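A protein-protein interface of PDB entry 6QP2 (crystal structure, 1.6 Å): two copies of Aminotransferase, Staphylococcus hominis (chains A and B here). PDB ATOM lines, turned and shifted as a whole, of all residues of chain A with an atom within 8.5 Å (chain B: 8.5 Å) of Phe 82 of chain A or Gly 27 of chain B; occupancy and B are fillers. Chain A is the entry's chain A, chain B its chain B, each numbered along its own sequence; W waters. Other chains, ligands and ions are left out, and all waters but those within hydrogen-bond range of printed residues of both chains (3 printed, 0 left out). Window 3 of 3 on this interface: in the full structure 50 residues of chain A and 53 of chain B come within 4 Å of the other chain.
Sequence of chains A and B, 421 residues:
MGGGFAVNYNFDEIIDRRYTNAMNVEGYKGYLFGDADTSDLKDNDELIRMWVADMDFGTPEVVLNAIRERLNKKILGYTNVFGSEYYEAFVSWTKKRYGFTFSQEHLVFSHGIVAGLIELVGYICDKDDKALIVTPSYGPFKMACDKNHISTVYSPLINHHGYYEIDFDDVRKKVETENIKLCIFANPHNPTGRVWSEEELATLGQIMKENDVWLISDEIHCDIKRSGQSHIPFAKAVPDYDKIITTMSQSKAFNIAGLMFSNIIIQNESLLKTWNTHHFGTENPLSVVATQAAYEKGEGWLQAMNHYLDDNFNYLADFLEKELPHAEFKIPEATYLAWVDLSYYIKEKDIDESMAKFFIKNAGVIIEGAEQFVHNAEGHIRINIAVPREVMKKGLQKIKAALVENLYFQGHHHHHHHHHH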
ATOM      1  N   TYR A  78      -2.995  18.254  25.182  1.00  0.00           N
ATOM      2  CA  TYR A  78      -1.871  17.374  25.343  1.00  0.00           C
ATOM      3  C   TYR A  78      -0.637  18.177  25.751  1.00  0.00           C
ATOM      4  O   TYR A  78      -0.350  19.232  25.181  1.00  0.00           O
ATOM      5  CB  TYR A  78      -1.593  16.564  24.072  1.00  0.00           C
ATOM      6  CG  TYR A  78      -2.646  15.519  23.797  1.00  0.00           C
ATOM      7  CD1 TYR A  78      -2.716  14.376  24.565  1.00  0.00           C
ATOM      8  CD2 TYR A  78      -3.626  15.716  22.835  1.00  0.00           C
ATOM      9  CE1 TYR A  78      -3.694  13.417  24.347  1.00  0.00           C
ATOM     10  CE2 TYR A  78      -4.615  14.771  22.604  1.00  0.00           C
ATOM     11  CZ  TYR A  78      -4.634  13.607  23.352  1.00  0.00           C
ATOM     12  OH  TYR A  78      -5.610  12.678  23.156  1.00  0.00           O
ATOM     13  N   THR A  79       0.094  17.630  26.721  1.00  0.00           N
ATOM     14  CA  THR A  79       1.229  18.312  27.331  1.00  0.00           C
ATOM     15  C   THR A  79       2.378  17.321  27.530  1.00  0.00           C
ATOM     16  O   THR A  79       2.165  16.177  27.886  1.00  0.00           O
ATOM     17  CB  THR A  79       0.789  18.910  28.676  1.00  0.00           C
ATOM     18  OG1 THR A  79      -0.374  19.684  28.408  1.00  0.00           O
ATOM     19  CG2 THR A  79       1.861  19.743  29.357  1.00  0.00           C
ATOM     20  N   ASN A  80       3.611  17.794  27.380  1.00  0.00           N
ATOM     21  CA  ASN A  80       4.797  17.058  27.798  1.00  0.00           C
ATOM     22  C   ASN A  80       5.779  18.093  28.349  1.00  0.00           C
ATOM     23  O   ASN A  80       5.577  19.282  28.157  1.00  0.00           O
ATOM     24  CB  ASN A  80       5.428  16.232  26.672  1.00  0.00           C
ATOM     25  CG  ASN A  80       4.719  14.918  26.406  1.00  0.00           C
ATOM     26  OD1 ASN A  80       4.850  13.959  27.176  1.00  0.00           O
ATOM     27  ND2 ASN A  80       3.971  14.866  25.314  1.00  0.00           N
ATOM     28  N   VAL A  81       6.791  17.628  29.070  1.00  0.00           N
ATOM     29  CA  VAL A  81       7.828  18.505  29.563  1.00  0.00           C
ATOM     30  C   VAL A  81       8.793  18.748  28.394  1.00  0.00           C
ATOM     31  O   VAL A  81       9.514  17.841  28.007  1.00  0.00           O
ATOM     32  CB  VAL A  81       8.529  17.880  30.783  1.00  0.00           C
ATOM     33  CG1 VAL A  81       9.632  18.778  31.318  1.00  0.00           C
ATOM     34  CG2 VAL A  81       7.527  17.552  31.879  1.00  0.00           C
ATOM     35  N   PHE A  82       8.713  19.945  27.797  1.00  0.00           N
ATOM     36  CA  PHE A  82       9.538  20.361  26.661  1.00  0.00           C
ATOM     37  C   PHE A  82      10.589  21.367  27.128  1.00  0.00           C
ATOM     38  O   PHE A  82      10.366  22.083  28.064  1.00  0.00           O
ATOM     39  CB  PHE A  82       8.657  20.986  25.581  1.00  0.00           C
ATOM     40  CG  PHE A  82       7.766  19.982  24.891  1.00  0.00           C
ATOM     41  CD1 PHE A  82       8.303  19.052  24.009  1.00  0.00           C
ATOM     42  CD2 PHE A  82       6.399  19.960  25.128  1.00  0.00           C
ATOM     43  CE1 PHE A  82       7.487  18.120  23.377  1.00  0.00           C
ATOM     44  CE2 PHE A  82       5.581  19.041  24.486  1.00  0.00           C
ATOM     45  CZ  PHE A  82       6.131  18.115  23.624  1.00  0.00           C
ATOM     46  N   GLY A  83      11.721  21.434  26.439  1.00  0.00           N
ATOM     47  CA  GLY A  83      12.721  22.435  26.787  1.00  0.00           C
ATOM     48  C   GLY A  83      13.407  22.046  28.083  1.00  0.00           C
ATOM     49  O   GLY A  83      13.374  20.873  28.494  1.00  0.00           O
ATOM     50  N   SER A  84      14.064  23.008  28.735  1.00  0.00           N
ATOM     51  CA  SER A  84      14.904  22.643  29.866  1.00  0.00           C
ATOM     52  C   SER A  84      14.501  23.411  31.129  1.00  0.00           C
ATOM     53  O   SER A  84      15.165  23.261  32.149  1.00  0.00           O
ATOM     54  CB  SER A  84      16.357  22.848  29.522  1.00  0.00           C
ATOM     55  OG  SER A  84      16.571  24.219  29.225  1.00  0.00           O
ATOM     56  N   GLU A  85      13.424  24.191  31.078  1.00  0.00           N
ATOM     57  CA  GLU A  85      13.034  25.042  32.197  1.00  0.00           C
ATOM     58  C   GLU A  85      12.671  24.181  33.414  1.00  0.00           C
ATOM     59  O   GLU A  85      13.079  24.490  34.499  1.00  0.00           O
ATOM     60  CB  GLU A  85      11.887  25.984  31.825  1.00  0.00           C
ATOM     61  CG  GLU A  85      12.317  27.086  30.857  1.00  0.00           C
ATOM     62  CD  GLU A  85      11.705  28.455  31.110  1.00  0.00           C
ATOM     63  OE1 GLU A  85      12.364  29.473  30.763  1.00  0.00           O
ATOM     64  OE2 GLU A  85      10.592  28.513  31.666  1.00  0.00           O
ATOM     65  N   TYR A  86      11.892  23.115  33.216  1.00  0.00           N
ATOM     66  CA  TYR A  86      11.510  22.246  34.335  1.00  0.00           C
ATOM     67  C   TYR A  86      12.753  21.573  34.924  1.00  0.00           C
ATOM     68  O   TYR A  86      12.990  21.604  36.138  1.00  0.00           O
ATOM     69  CB  TYR A  86      10.472  21.199  33.922  1.00  0.00           C
ATOM     70  CG  TYR A  86      10.142  20.269  35.063  1.00  0.00           C
ATOM     71  CD1 TYR A  86      10.896  19.142  35.324  1.00  0.00           C
ATOM     72  CD2 TYR A  86       9.117  20.583  35.946  1.00  0.00           C
ATOM     73  CE1 TYR A  86      10.576  18.281  36.365  1.00  0.00           C
ATOM     74  CE2 TYR A  86       8.817  19.758  37.024  1.00  0.00           C
ATOM     75  CZ  TYR A  86       9.546  18.603  37.232  1.00  0.00           C
ATOM     76  OH  TYR A  86       9.261  17.789  38.297  1.00  0.00           O
ATOM     77  N   TYR A  87      13.575  20.961  34.053  1.00  0.00           N
ATOM     78  CA  TYR A  87      14.815  20.390  34.462  1.00  0.00           C
ATOM     79  C   TYR A  87      15.644  21.412  35.253  1.00  0.00           C
ATOM     80  O   TYR A  87      16.167  21.079  36.319  1.00  0.00           O
ATOM     81  CB  TYR A  87      15.636  19.881  33.277  1.00  0.00           C
ATOM     82  CG  TYR A  87      17.071  19.604  33.626  1.00  0.00           C
ATOM     83  CD1 TYR A  87      17.427  18.475  34.332  1.00  0.00           C
ATOM     84  CD2 TYR A  87      18.069  20.492  33.281  1.00  0.00           C
ATOM     85  CE1 TYR A  87      18.735  18.236  34.702  1.00  0.00           C
ATOM     86  CE2 TYR A  87      19.390  20.244  33.591  1.00  0.00           C
ATOM     87  CZ  TYR A  87      19.726  19.116  34.312  1.00  0.00           C
ATOM     88  OH  TYR A  87      21.023  18.869  34.613  1.00  0.00           O
ATOM     89  N   GLN A 104      19.972  15.934  32.489  1.00  0.00           N
ATOM     90  CA  GLN A 104      18.611  16.100  31.962  1.00  0.00           C
ATOM     91  C   GLN A 104      18.181  14.832  31.207  1.00  0.00           C
ATOM     92  O   GLN A 104      17.011  14.472  31.280  1.00  0.00           O
ATOM     93  CB  GLN A 104      18.498  17.371  31.106  1.00  0.00           C
ATOM     94  CG  GLN A 104      17.149  17.555  30.431  1.00  0.00           C
ATOM     95  CD  GLN A 104      17.071  18.807  29.589  1.00  0.00           C
ATOM     96  OE1 GLN A 104      18.076  19.480  29.354  1.00  0.00           O
ATOM     97  NE2 GLN A 104      15.867  19.157  29.174  1.00  0.00           N
ATOM     98  N   PHE A 109       9.354  10.770  33.842  1.00  0.00           N
ATOM     99  CA  PHE A 109       8.249  11.123  34.718  1.00  0.00           C
ATOM    100  C   PHE A 109       7.271   9.961  34.860  1.00  0.00           C
ATOM    101  O   PHE A 109       7.071   9.196  33.917  1.00  0.00           O
ATOM    102  CB  PHE A 109       7.537  12.362  34.173  1.00  0.00           C
ATOM    103  CG  PHE A 109       8.495  13.477  33.871  1.00  0.00           C
ATOM    104  CD1 PHE A 109       9.118  14.155  34.909  1.00  0.00           C
ATOM    105  CD2 PHE A 109       8.881  13.762  32.565  1.00  0.00           C
ATOM    106  CE1 PHE A 109      10.035  15.160  34.642  1.00  0.00           C
ATOM    107  CE2 PHE A 109       9.799  14.770  32.300  1.00  0.00           C
ATOM    108  CZ  PHE A 109      10.371  15.468  33.336  1.00  0.00           C
ATOM    109  N   GLY A 281       3.873   7.878  27.828  1.00  0.00           N
ATOM    110  CA  GLY A 281       3.938   8.998  28.778  1.00  0.00           C
ATOM    111  C   GLY A 281       3.468  10.306  28.162  1.00  0.00           C
ATOM    112  O   GLY A 281       4.050  10.793  27.193  1.00  0.00           O
ATOM    113  N   THR A 282       2.400  10.866  28.740  1.00  0.00           N
ATOM    114  CA  THR A 282       1.939  12.231  28.465  1.00  0.00           C
ATOM    115  C   THR A 282       1.636  12.864  29.832  1.00  0.00           C
ATOM    116  O   THR A 282       1.385  12.132  30.780  1.00  0.00           O
ATOM    117  CB  THR A 282       0.790  12.184  27.448  1.00  0.00           C
ATOM    118  OG1 THR A 282       0.437  13.523  27.101  1.00  0.00           O
ATOM    119  CG2 THR A 282      -0.422  11.431  27.959  1.00  0.00           C
ATOM    120  N   GLU A 283       1.689  14.197  29.958  1.00  0.00           N
ATOM    121  CA  GLU A 283       1.677  14.805  31.312  1.00  0.00           C
ATOM    122  C   GLU A 283       0.455  15.704  31.486  1.00  0.00           C
ATOM    123  O   GLU A 283      -0.193  16.128  30.523  1.00  0.00           O
ATOM    124  CB  GLU A 283       2.983  15.549  31.576  1.00  0.00           C
ATOM    125  CG  GLU A 283       4.228  14.701  31.397  1.00  0.00           C
ATOM    126  CD  GLU A 283       4.204  13.359  32.107  1.00  0.00           C
ATOM    127  OE1 GLU A 283       4.938  12.440  31.652  1.00  0.00           O
ATOM    128  OE2 GLU A 283       3.429  13.216  33.097  1.00  0.00           O
ATOM    129  N   VAL A 288       2.201  19.677  36.119  1.00  0.00           N
ATOM    130  CA  VAL A 288       3.552  20.091  35.798  1.00  0.00           C
ATOM    131  C   VAL A 288       3.772  21.515  36.307  1.00  0.00           C
ATOM    132  O   VAL A 288       4.811  21.794  36.948  1.00  0.00           O
ATOM    133  CB  VAL A 288       3.859  19.986  34.294  1.00  0.00           C
ATOM    134  CG1 VAL A 288       5.202  20.615  33.978  1.00  0.00           C
ATOM    135  CG2 VAL A 288       3.866  18.533  33.843  1.00  0.00           C
ATOM    136  N   GLN A 292       6.527  22.475  39.172  1.00  0.00           N
ATOM    137  CA  GLN A 292       7.547  23.418  38.783  1.00  0.00           C
ATOM    138  C   GLN A 292       7.518  24.627  39.722  1.00  0.00           C
ATOM    139  O   GLN A 292       8.596  25.076  40.134  1.00  0.00           O
ATOM    140  CB  GLN A 292       7.386  23.862  37.333  1.00  0.00           C
ATOM    141  CG  GLN A 292       8.612  24.590  36.805  1.00  0.00           C
ATOM    142  CD  GLN A 292       8.630  24.722  35.294  1.00  0.00           C
ATOM    143  OE1 GLN A 292       8.163  23.854  34.568  1.00  0.00           O
ATOM    144  NE2 GLN A 292       9.215  25.802  34.796  1.00  0.00           N
ATOM    145  N   THR B  20       3.194  26.829  26.954  1.00  0.00           N
ATOM    146  CA  THR B  20       2.269  25.976  27.736  1.00  0.00           C
ATOM    147  C   THR B  20       2.668  24.497  27.680  1.00  0.00           C
ATOM    148  O   THR B  20       1.903  23.654  28.148  1.00  0.00           O
ATOM    149  CB  THR B  20       0.806  26.118  27.292  1.00  0.00           C
ATOM    150  OG1 THR B  20       0.618  25.723  25.930  1.00  0.00           O
ATOM    151  CG2 THR B  20       0.279  27.522  27.481  1.00  0.00           C
ATOM    152  N   ASN B  21       3.845  24.180  27.128  1.00  0.00           N
ATOM    153  CA  ASN B  21       4.299  22.803  27.042  1.00  0.00           C
ATOM    154  C   ASN B  21       3.291  21.984  26.225  1.00  0.00           C
ATOM    155  O   ASN B  21       3.109  20.762  26.482  1.00  0.00           O
ATOM    156  CB  ASN B  21       4.504  22.207  28.439  1.00  0.00           C
ATOM    157  CG  ASN B  21       5.899  22.409  28.988  1.00  0.00           C
ATOM    158  OD1 ASN B  21       6.879  22.293  28.254  1.00  0.00           O
ATOM    159  ND2 ASN B  21       5.995  22.633  30.292  1.00  0.00           N
ATOM    160  N   ALA B  22       2.612  22.649  25.286  1.00  0.00           N
ATOM    161  CA  ALA B  22       1.574  21.988  24.450  1.00  0.00           C
ATOM    162  C   ALA B  22       2.286  21.106  23.414  1.00  0.00           C
ATOM    163  O   ALA B  22       3.136  21.586  22.644  1.00  0.00           O
ATOM    164  CB  ALA B  22       0.670  23.000  23.789  1.00  0.00           C
ATOM    165  N   MET B  23       1.952  19.813  23.406  1.00  0.00           N
ATOM    166  CA  MET B  23       2.439  18.893  22.371  1.00  0.00           C
ATOM    167  C   MET B  23       2.180  19.504  20.984  1.00  0.00           C
ATOM    168  O   MET B  23       3.056  19.463  20.098  1.00  0.00           O
ATOM    169  CB  MET B  23       1.734  17.536  22.484  1.00  0.00           C
ATOM    170  CG  MET B  23       2.261  16.486  21.529  1.00  0.00           C
ATOM    171  SD  MET B  23       1.232  14.993  21.535  1.00  0.00           S
ATOM    172  CE  MET B  23       2.071  14.014  22.781  1.00  0.00           C
ATOM    173  N   ASN B  24       0.982  20.078  20.811  1.00  0.00           N
ATOM    174  CA  ASN B  24       0.532  20.695  19.518  1.00  0.00           C
ATOM    175  C   ASN B  24       1.592  21.683  18.977  1.00  0.00           C
ATOM    176  O   ASN B  24       1.890  21.675  17.777  1.00  0.00           O
ATOM    177  CB  ASN B  24      -0.847  21.350  19.671  1.00  0.00           C
ATOM    178  CG  ASN B  24      -1.598  21.517  18.365  1.00  0.00           C
ATOM    179  OD1 ASN B  24      -1.021  21.935  17.369  1.00  0.00           O
ATOM    180  ND2 ASN B  24      -2.875  21.176  18.341  1.00  0.00           N
ATOM    181  N   VAL B  25       2.180  22.484  19.879  1.00  0.00           N
ATOM    182  CA  VAL B  25       3.109  23.585  19.544  1.00  0.00           C
ATOM    183  C   VAL B  25       4.555  23.079  19.526  1.00  0.00           C
ATOM    184  O   VAL B  25       5.321  23.511  18.662  1.00  0.00           O
ATOM    185  CB  VAL B  25       2.972  24.764  20.529  1.00  0.00           C
ATOM    186  CG1 VAL B  25       4.076  25.806  20.342  1.00  0.00           C
ATOM    187  CG2 VAL B  25       1.604  25.414  20.454  1.00  0.00           C
ATOM    188  N   GLU B  26       4.948  22.226  20.484  1.00  0.00           N
ATOM    189  CA  GLU B  26       6.389  21.948  20.739  1.00  0.00           C
ATOM    190  C   GLU B  26       6.853  20.624  20.112  1.00  0.00           C
ATOM    191  O   GLU B  26       8.031  20.441  19.929  1.00  0.00           O
ATOM    192  CB  GLU B  26       6.715  21.879  22.241  1.00  0.00           C
ATOM    193  CG  GLU B  26       6.134  23.008  23.089  1.00  0.00           C
ATOM    194  CD  GLU B  26       6.548  24.443  22.782  1.00  0.00           C
ATOM    195  OE1 GLU B  26       7.569  24.636  22.090  1.00  0.00           O
ATOM    196  OE2 GLU B  26       5.816  25.380  23.221  1.00  0.00           O
ATOM    197  N   GLY B  27       5.941  19.672  19.873  1.00  0.00           N
ATOM    198  CA  GLY B  27       6.316  18.254  19.863  1.00  0.00           C
ATOM    199  C   GLY B  27       6.122  17.531  18.534  1.00  0.00           C
ATOM    200  O   GLY B  27       6.155  16.286  18.499  1.00  0.00           O
ATOM    201  N   TYR B  28       5.943  18.277  17.438  1.00  0.00           N
ATOM    202  CA  TYR B  28       5.555  17.673  16.136  1.00  0.00           C
ATOM    203  C   TYR B  28       6.680  16.763  15.594  1.00  0.00           C
ATOM    204  O   TYR B  28       6.395  15.718  14.957  1.00  0.00           O
ATOM    205  CB  TYR B  28       5.101  18.749  15.138  1.00  0.00           C
ATOM    206  CG  TYR B  28       6.063  19.897  14.940  1.00  0.00           C
ATOM    207  CD1 TYR B  28       7.147  19.786  14.084  1.00  0.00           C
ATOM    208  CD2 TYR B  28       5.882  21.100  15.603  1.00  0.00           C
ATOM    209  CE1 TYR B  28       8.036  20.835  13.901  1.00  0.00           C
ATOM    210  CE2 TYR B  28       6.758  22.160  15.432  1.00  0.00           C
ATOM    211  CZ  TYR B  28       7.841  22.028  14.579  1.00  0.00           C
ATOM    212  OH  TYR B  28       8.705  23.074  14.414  1.00  0.00           O
ATOM    213  N   LYS B  29       7.943  17.108  15.880  1.00  0.00           N
ATOM    214  CA  LYS B  29       9.105  16.375  15.325  1.00  0.00           C
ATOM    215  C   LYS B  29       9.169  14.946  15.891  1.00  0.00           C
ATOM    216  O   LYS B  29       9.282  13.987  15.120  1.00  0.00           O
ATOM    217  CB  LYS B  29      10.395  17.162  15.572  1.00  0.00           C
ATOM    218  CG  LYS B  29      10.497  18.447  14.760  1.00  0.00           C
ATOM    219  CD  LYS B  29      11.268  19.555  15.445  1.00  0.00           C
ATOM    220  CE  LYS B  29      12.760  19.469  15.204  1.00  0.00           C
ATOM    221  NZ  LYS B  29      13.151  20.223  13.987  1.00  0.00           N
ATOM    222  N   GLY B  30       9.083  14.815  17.224  1.00  0.00           N
ATOM    223  CA  GLY B  30       9.120  13.513  17.915  1.00  0.00           C
ATOM    224  C   GLY B  30       7.904  12.651  17.590  1.00  0.00           C
ATOM    225  O   GLY B  30       8.028  11.436  17.412  1.00  0.00           O
ATOM    226  N   TYR B  31       6.726  13.281  17.489  1.00  0.00           N
ATOM    227  CA  TYR B  31       5.448  12.571  17.262  1.00  0.00           C
ATOM    228  C   TYR B  31       5.372  12.060  15.814  1.00  0.00           C
ATOM    229  O   TYR B  31       5.046  10.901  15.594  1.00  0.00           O
ATOM    230  CB  TYR B  31       4.279  13.487  17.637  1.00  0.00           C
ATOM    231  CG  TYR B  31       2.883  12.937  17.452  1.00  0.00           C
ATOM    232  CD1 TYR B  31       2.407  12.586  16.196  1.00  0.00           C
ATOM    233  CD2 TYR B  31       1.997  12.862  18.521  1.00  0.00           C
ATOM    234  CE1 TYR B  31       1.113  12.123  16.013  1.00  0.00           C
ATOM    235  CE2 TYR B  31       0.695  12.409  18.354  1.00  0.00           C
ATOM    236  CZ  TYR B  31       0.252  12.037  17.093  1.00  0.00           C
ATOM    237  OH  TYR B  31      -1.022  11.592  16.890  1.00  0.00           O
ATOM    238  N   LEU B  32       5.664  12.927  14.838  1.00  0.00           N
ATOM    239  CA  LEU B  32       5.450  12.618  13.410  1.00  0.00           C
ATOM    240  C   LEU B  32       6.639  11.887  12.767  1.00  0.00           C
ATOM    241  O   LEU B  32       6.433  11.261  11.737  1.00  0.00           O
ATOM    242  CB  LEU B  32       5.174  13.910  12.635  1.00  0.00           C
ATOM    243  CG  LEU B  32       3.838  14.593  12.934  1.00  0.00           C
ATOM    244  CD1 LEU B  32       3.881  16.051  12.498  1.00  0.00           C
ATOM    245  CD2 LEU B  32       2.688  13.859  12.252  1.00  0.00           C
ATOM    246  N   PHE B  33       7.859  11.986  13.322  1.00  0.00           N
ATOM    247  CA  PHE B  33       9.089  11.584  12.565  1.00  0.00           C
ATOM    248  C   PHE B  33       9.984  10.611  13.353  1.00  0.00           C
ATOM    249  O   PHE B  33      10.074  10.632  14.579  1.00  0.00           O
ATOM    250  CB  PHE B  33       9.852  12.838  12.119  1.00  0.00           C
ATOM    251  CG  PHE B  33       9.044  13.793  11.270  1.00  0.00           C
ATOM    252  CD1 PHE B  33       8.397  13.351  10.120  1.00  0.00           C
ATOM    253  CD2 PHE B  33       8.931  15.135  11.612  1.00  0.00           C
ATOM    254  CE1 PHE B  33       7.649  14.228   9.347  1.00  0.00           C
ATOM    255  CE2 PHE B  33       8.185  16.009  10.835  1.00  0.00           C
ATOM    256  CZ  PHE B  33       7.545  15.553   9.705  1.00  0.00           C
ATOM    257  N   ARG B  49      -0.973  25.034  12.706  1.00  0.00           N
ATOM    258  CA  ARG B  49      -1.076  23.732  13.357  1.00  0.00           C
ATOM    259  C   ARG B  49      -2.471  23.144  13.104  1.00  0.00           C
ATOM    260  O   ARG B  49      -3.489  23.679  13.564  1.00  0.00           O
ATOM    261  CB  ARG B  49      -0.830  23.880  14.860  1.00  0.00           C
ATOM    262  CG  ARG B  49       0.512  24.487  15.244  1.00  0.00           C
ATOM    263  CD  ARG B  49       0.562  24.820  16.728  1.00  0.00           C
ATOM    264  NE  ARG B  49      -0.239  25.978  17.121  1.00  0.00           N
ATOM    265  CZ  ARG B  49      -1.484  25.936  17.602  1.00  0.00           C
ATOM    266  NH1 ARG B  49      -2.129  27.066  17.834  1.00  0.00           N
ATOM    267  NH2 ARG B  49      -2.090  24.779  17.836  1.00  0.00           N
ATOM    268  N   TRP B  51      -2.882  19.387  13.152  1.00  0.00           N
ATOM    269  CA  TRP B  51      -2.361  18.001  13.195  1.00  0.00           C
ATOM    270  C   TRP B  51      -2.979  17.209  14.359  1.00  0.00           C
ATOM    271  O   TRP B  51      -4.042  16.617  14.164  1.00  0.00           O
ATOM    272  CB  TRP B  51      -0.828  17.931  13.137  1.00  0.00           C
ATOM    273  CG  TRP B  51      -0.068  18.509  14.296  1.00  0.00           C
ATOM    274  CD1 TRP B  51      -0.001  19.815  14.689  1.00  0.00           C
ATOM    275  CD2 TRP B  51       0.800  17.780  15.178  1.00  0.00           C
ATOM    276  NE1 TRP B  51       0.834  19.946  15.770  1.00  0.00           N
ATOM    277  CE2 TRP B  51       1.346  18.714  16.088  1.00  0.00           C
ATOM    278  CE3 TRP B  51       1.138  16.424  15.304  1.00  0.00           C
ATOM    279  CZ2 TRP B  51       2.203  18.320  17.118  1.00  0.00           C
ATOM    280  CZ3 TRP B  51       1.978  16.038  16.327  1.00  0.00           C
ATOM    281  CH2 TRP B  51       2.505  16.979  17.217  1.00  0.00           C
ATOM    282  N   VAL B  52      -2.378  17.257  15.555  1.00  0.00           N
ATOM    283  CA  VAL B  52      -2.774  16.399  16.680  1.00  0.00           C
ATOM    284  C   VAL B  52      -4.154  16.846  17.186  1.00  0.00           C
ATOM    285  O   VAL B  52      -4.492  18.040  17.158  1.00  0.00           O
ATOM    286  CB  VAL B  52      -1.715  16.396  17.806  1.00  0.00           C
ATOM    287  CG1 VAL B  52      -1.572  17.764  18.451  1.00  0.00           C
ATOM    288  CG2 VAL B  52      -1.994  15.315  18.853  1.00  0.00           C
ATOM    289  N   ILE B 366       1.225  22.090   9.557  1.00  0.00           N
ATOM    290  CA  ILE B 366       1.422  20.772  10.154  1.00  0.00           C
ATOM    291  C   ILE B 366       0.102  20.008  10.055  1.00  0.00           C
ATOM    292  O   ILE B 366      -0.897  20.417  10.639  1.00  0.00           O
ATOM    293  CB  ILE B 366       1.886  20.845  11.628  1.00  0.00           C
ATOM    294  CG1 ILE B 366       2.805  22.038  11.914  1.00  0.00           C
ATOM    295  CG2 ILE B 366       2.536  19.516  12.038  1.00  0.00           C
ATOM    296  CD1 ILE B 366       3.237  22.127  13.368  1.00  0.00           C
HETATM  297  O   HOH W   1       8.480  23.691  31.792  1.00  0.00           O
HETATM  298  O   HOH W   2      -1.258  19.997  22.596  1.00  0.00           O
HETATM  299  O   HOH W   3      -0.290  22.270  27.575  1.00  0.00           O
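The backbone NH of Met 23 of chain B lies within hydrogen-bond range of the backbone carbonyl oxygen of Tyr 78 of chain A (3.0 Å). The backbone carbonyl oxygen (O) of Asn 21 of chain B sits at hydrogen-bond distance from the backbone NH (N) of Asn 80 of chain A (3.1 Å). The backbone NH of Phe 82 of chain A lies within hydrogen-bond range of the side-chain amide oxygen of Asn 21 of chain B (3.0 Å).
The backbone carbonyl oxygen (O) of Thr 79 of chain A is in hydrogen-bond range of the side-chain hydroxyl (OG1) of Thr 282 of chain A (3.3 Å). O of Thr 79 of chain A sits at hydrogen-bond distance from N of Glu 283 of chain A (2.9 Å). The backbone carbonyl oxygen (O) of Gly 281 of chain A sits close to the side-chain amide oxygen (OD1) of Asn 80 of chain A.
Among the printed residues, merely in contact across the chains: Thr 79 of chain A with Asn 21 of chain B, Asn 80 of chain A with Met 23 of chain B, Phe 82 of chain A with Glu 26 of chain B, Tyr 78 of chain A with Ala 22 of chain B, Phe 82 of chain A with Gly 27 of chain B, Phe 82 of chain A with Met 23 of chain B, Phe 82 of chain A with Ala 22 of chain B and Tyr 78 of chain A with Asn 21 of chain B.
Printed residues of chain B within 4 Å of Phe 82 of chain A: Asn 21 (3.0 Å), Ala 22 (3.98 Å), Met 23 (3.8 Å), Glu 26 (3.4 Å) and Gly 27 (3.7 Å). Of the printed residues of chain B, Tyr 78 of chain A touches Asn 21, Ala 22 and Met 23. Printed residues of chain B within 4 Å of Asn 80 of chain A: Asn 21 and Met 23. Of the printed residues of chain A, Asn 21 of chain B touches Tyr 78, Thr 79, Asn 80 and Phe 82. The nearest printed residue of chain B that does not touch Phe 82 of chain A is Asn 24 of chain B (6.0 Å). The nearest residue of chain A that does not touch Gly 27 of chain B is Asn 80 of chain A (6.8 Å). The nearest printed residue of chain A that does not touch Asn 21 of chain B is Val 81 of chain A (4.03 Å).
Hydrophobic or aromatic side chains of chain A that line the printed part of chain B: Tyr 78 and Phe 82. Along chain A the printed residues that touch a printed residue of chain B span positions 78 to 82. Of the 18 printed residues of chain B, 5 touch a printed residue of chain A. Printed residues of chain B that touch a printed residue of chain A: Asn 21, Ala 22, Met 23, Glu 26 and Gly 27. Hydrophobic or aromatic side chains of chain B that line the printed part of chain A: Met 23. Along chain B the printed residues that touch a printed residue of chain A span positions 21 to 27.
No position is printed for both chains. Of the 11 pairs that touch across the chains among the printed residues, none has its exchanged pair printed and touching as well.
Water W3 bridges O of Thr 20 of chain B and OG1 of Thr 79 of chain A. Water W2 lies within hydrogen-bond range of the backbone carbonyl oxygen (O) of Tyr 78 of chain A (2.8 Å), the backbone NH (N) of Asn 24 of chain B (2.9 Å) and the backbone NH (N) of Met 23 of chain B (3.3 Å).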
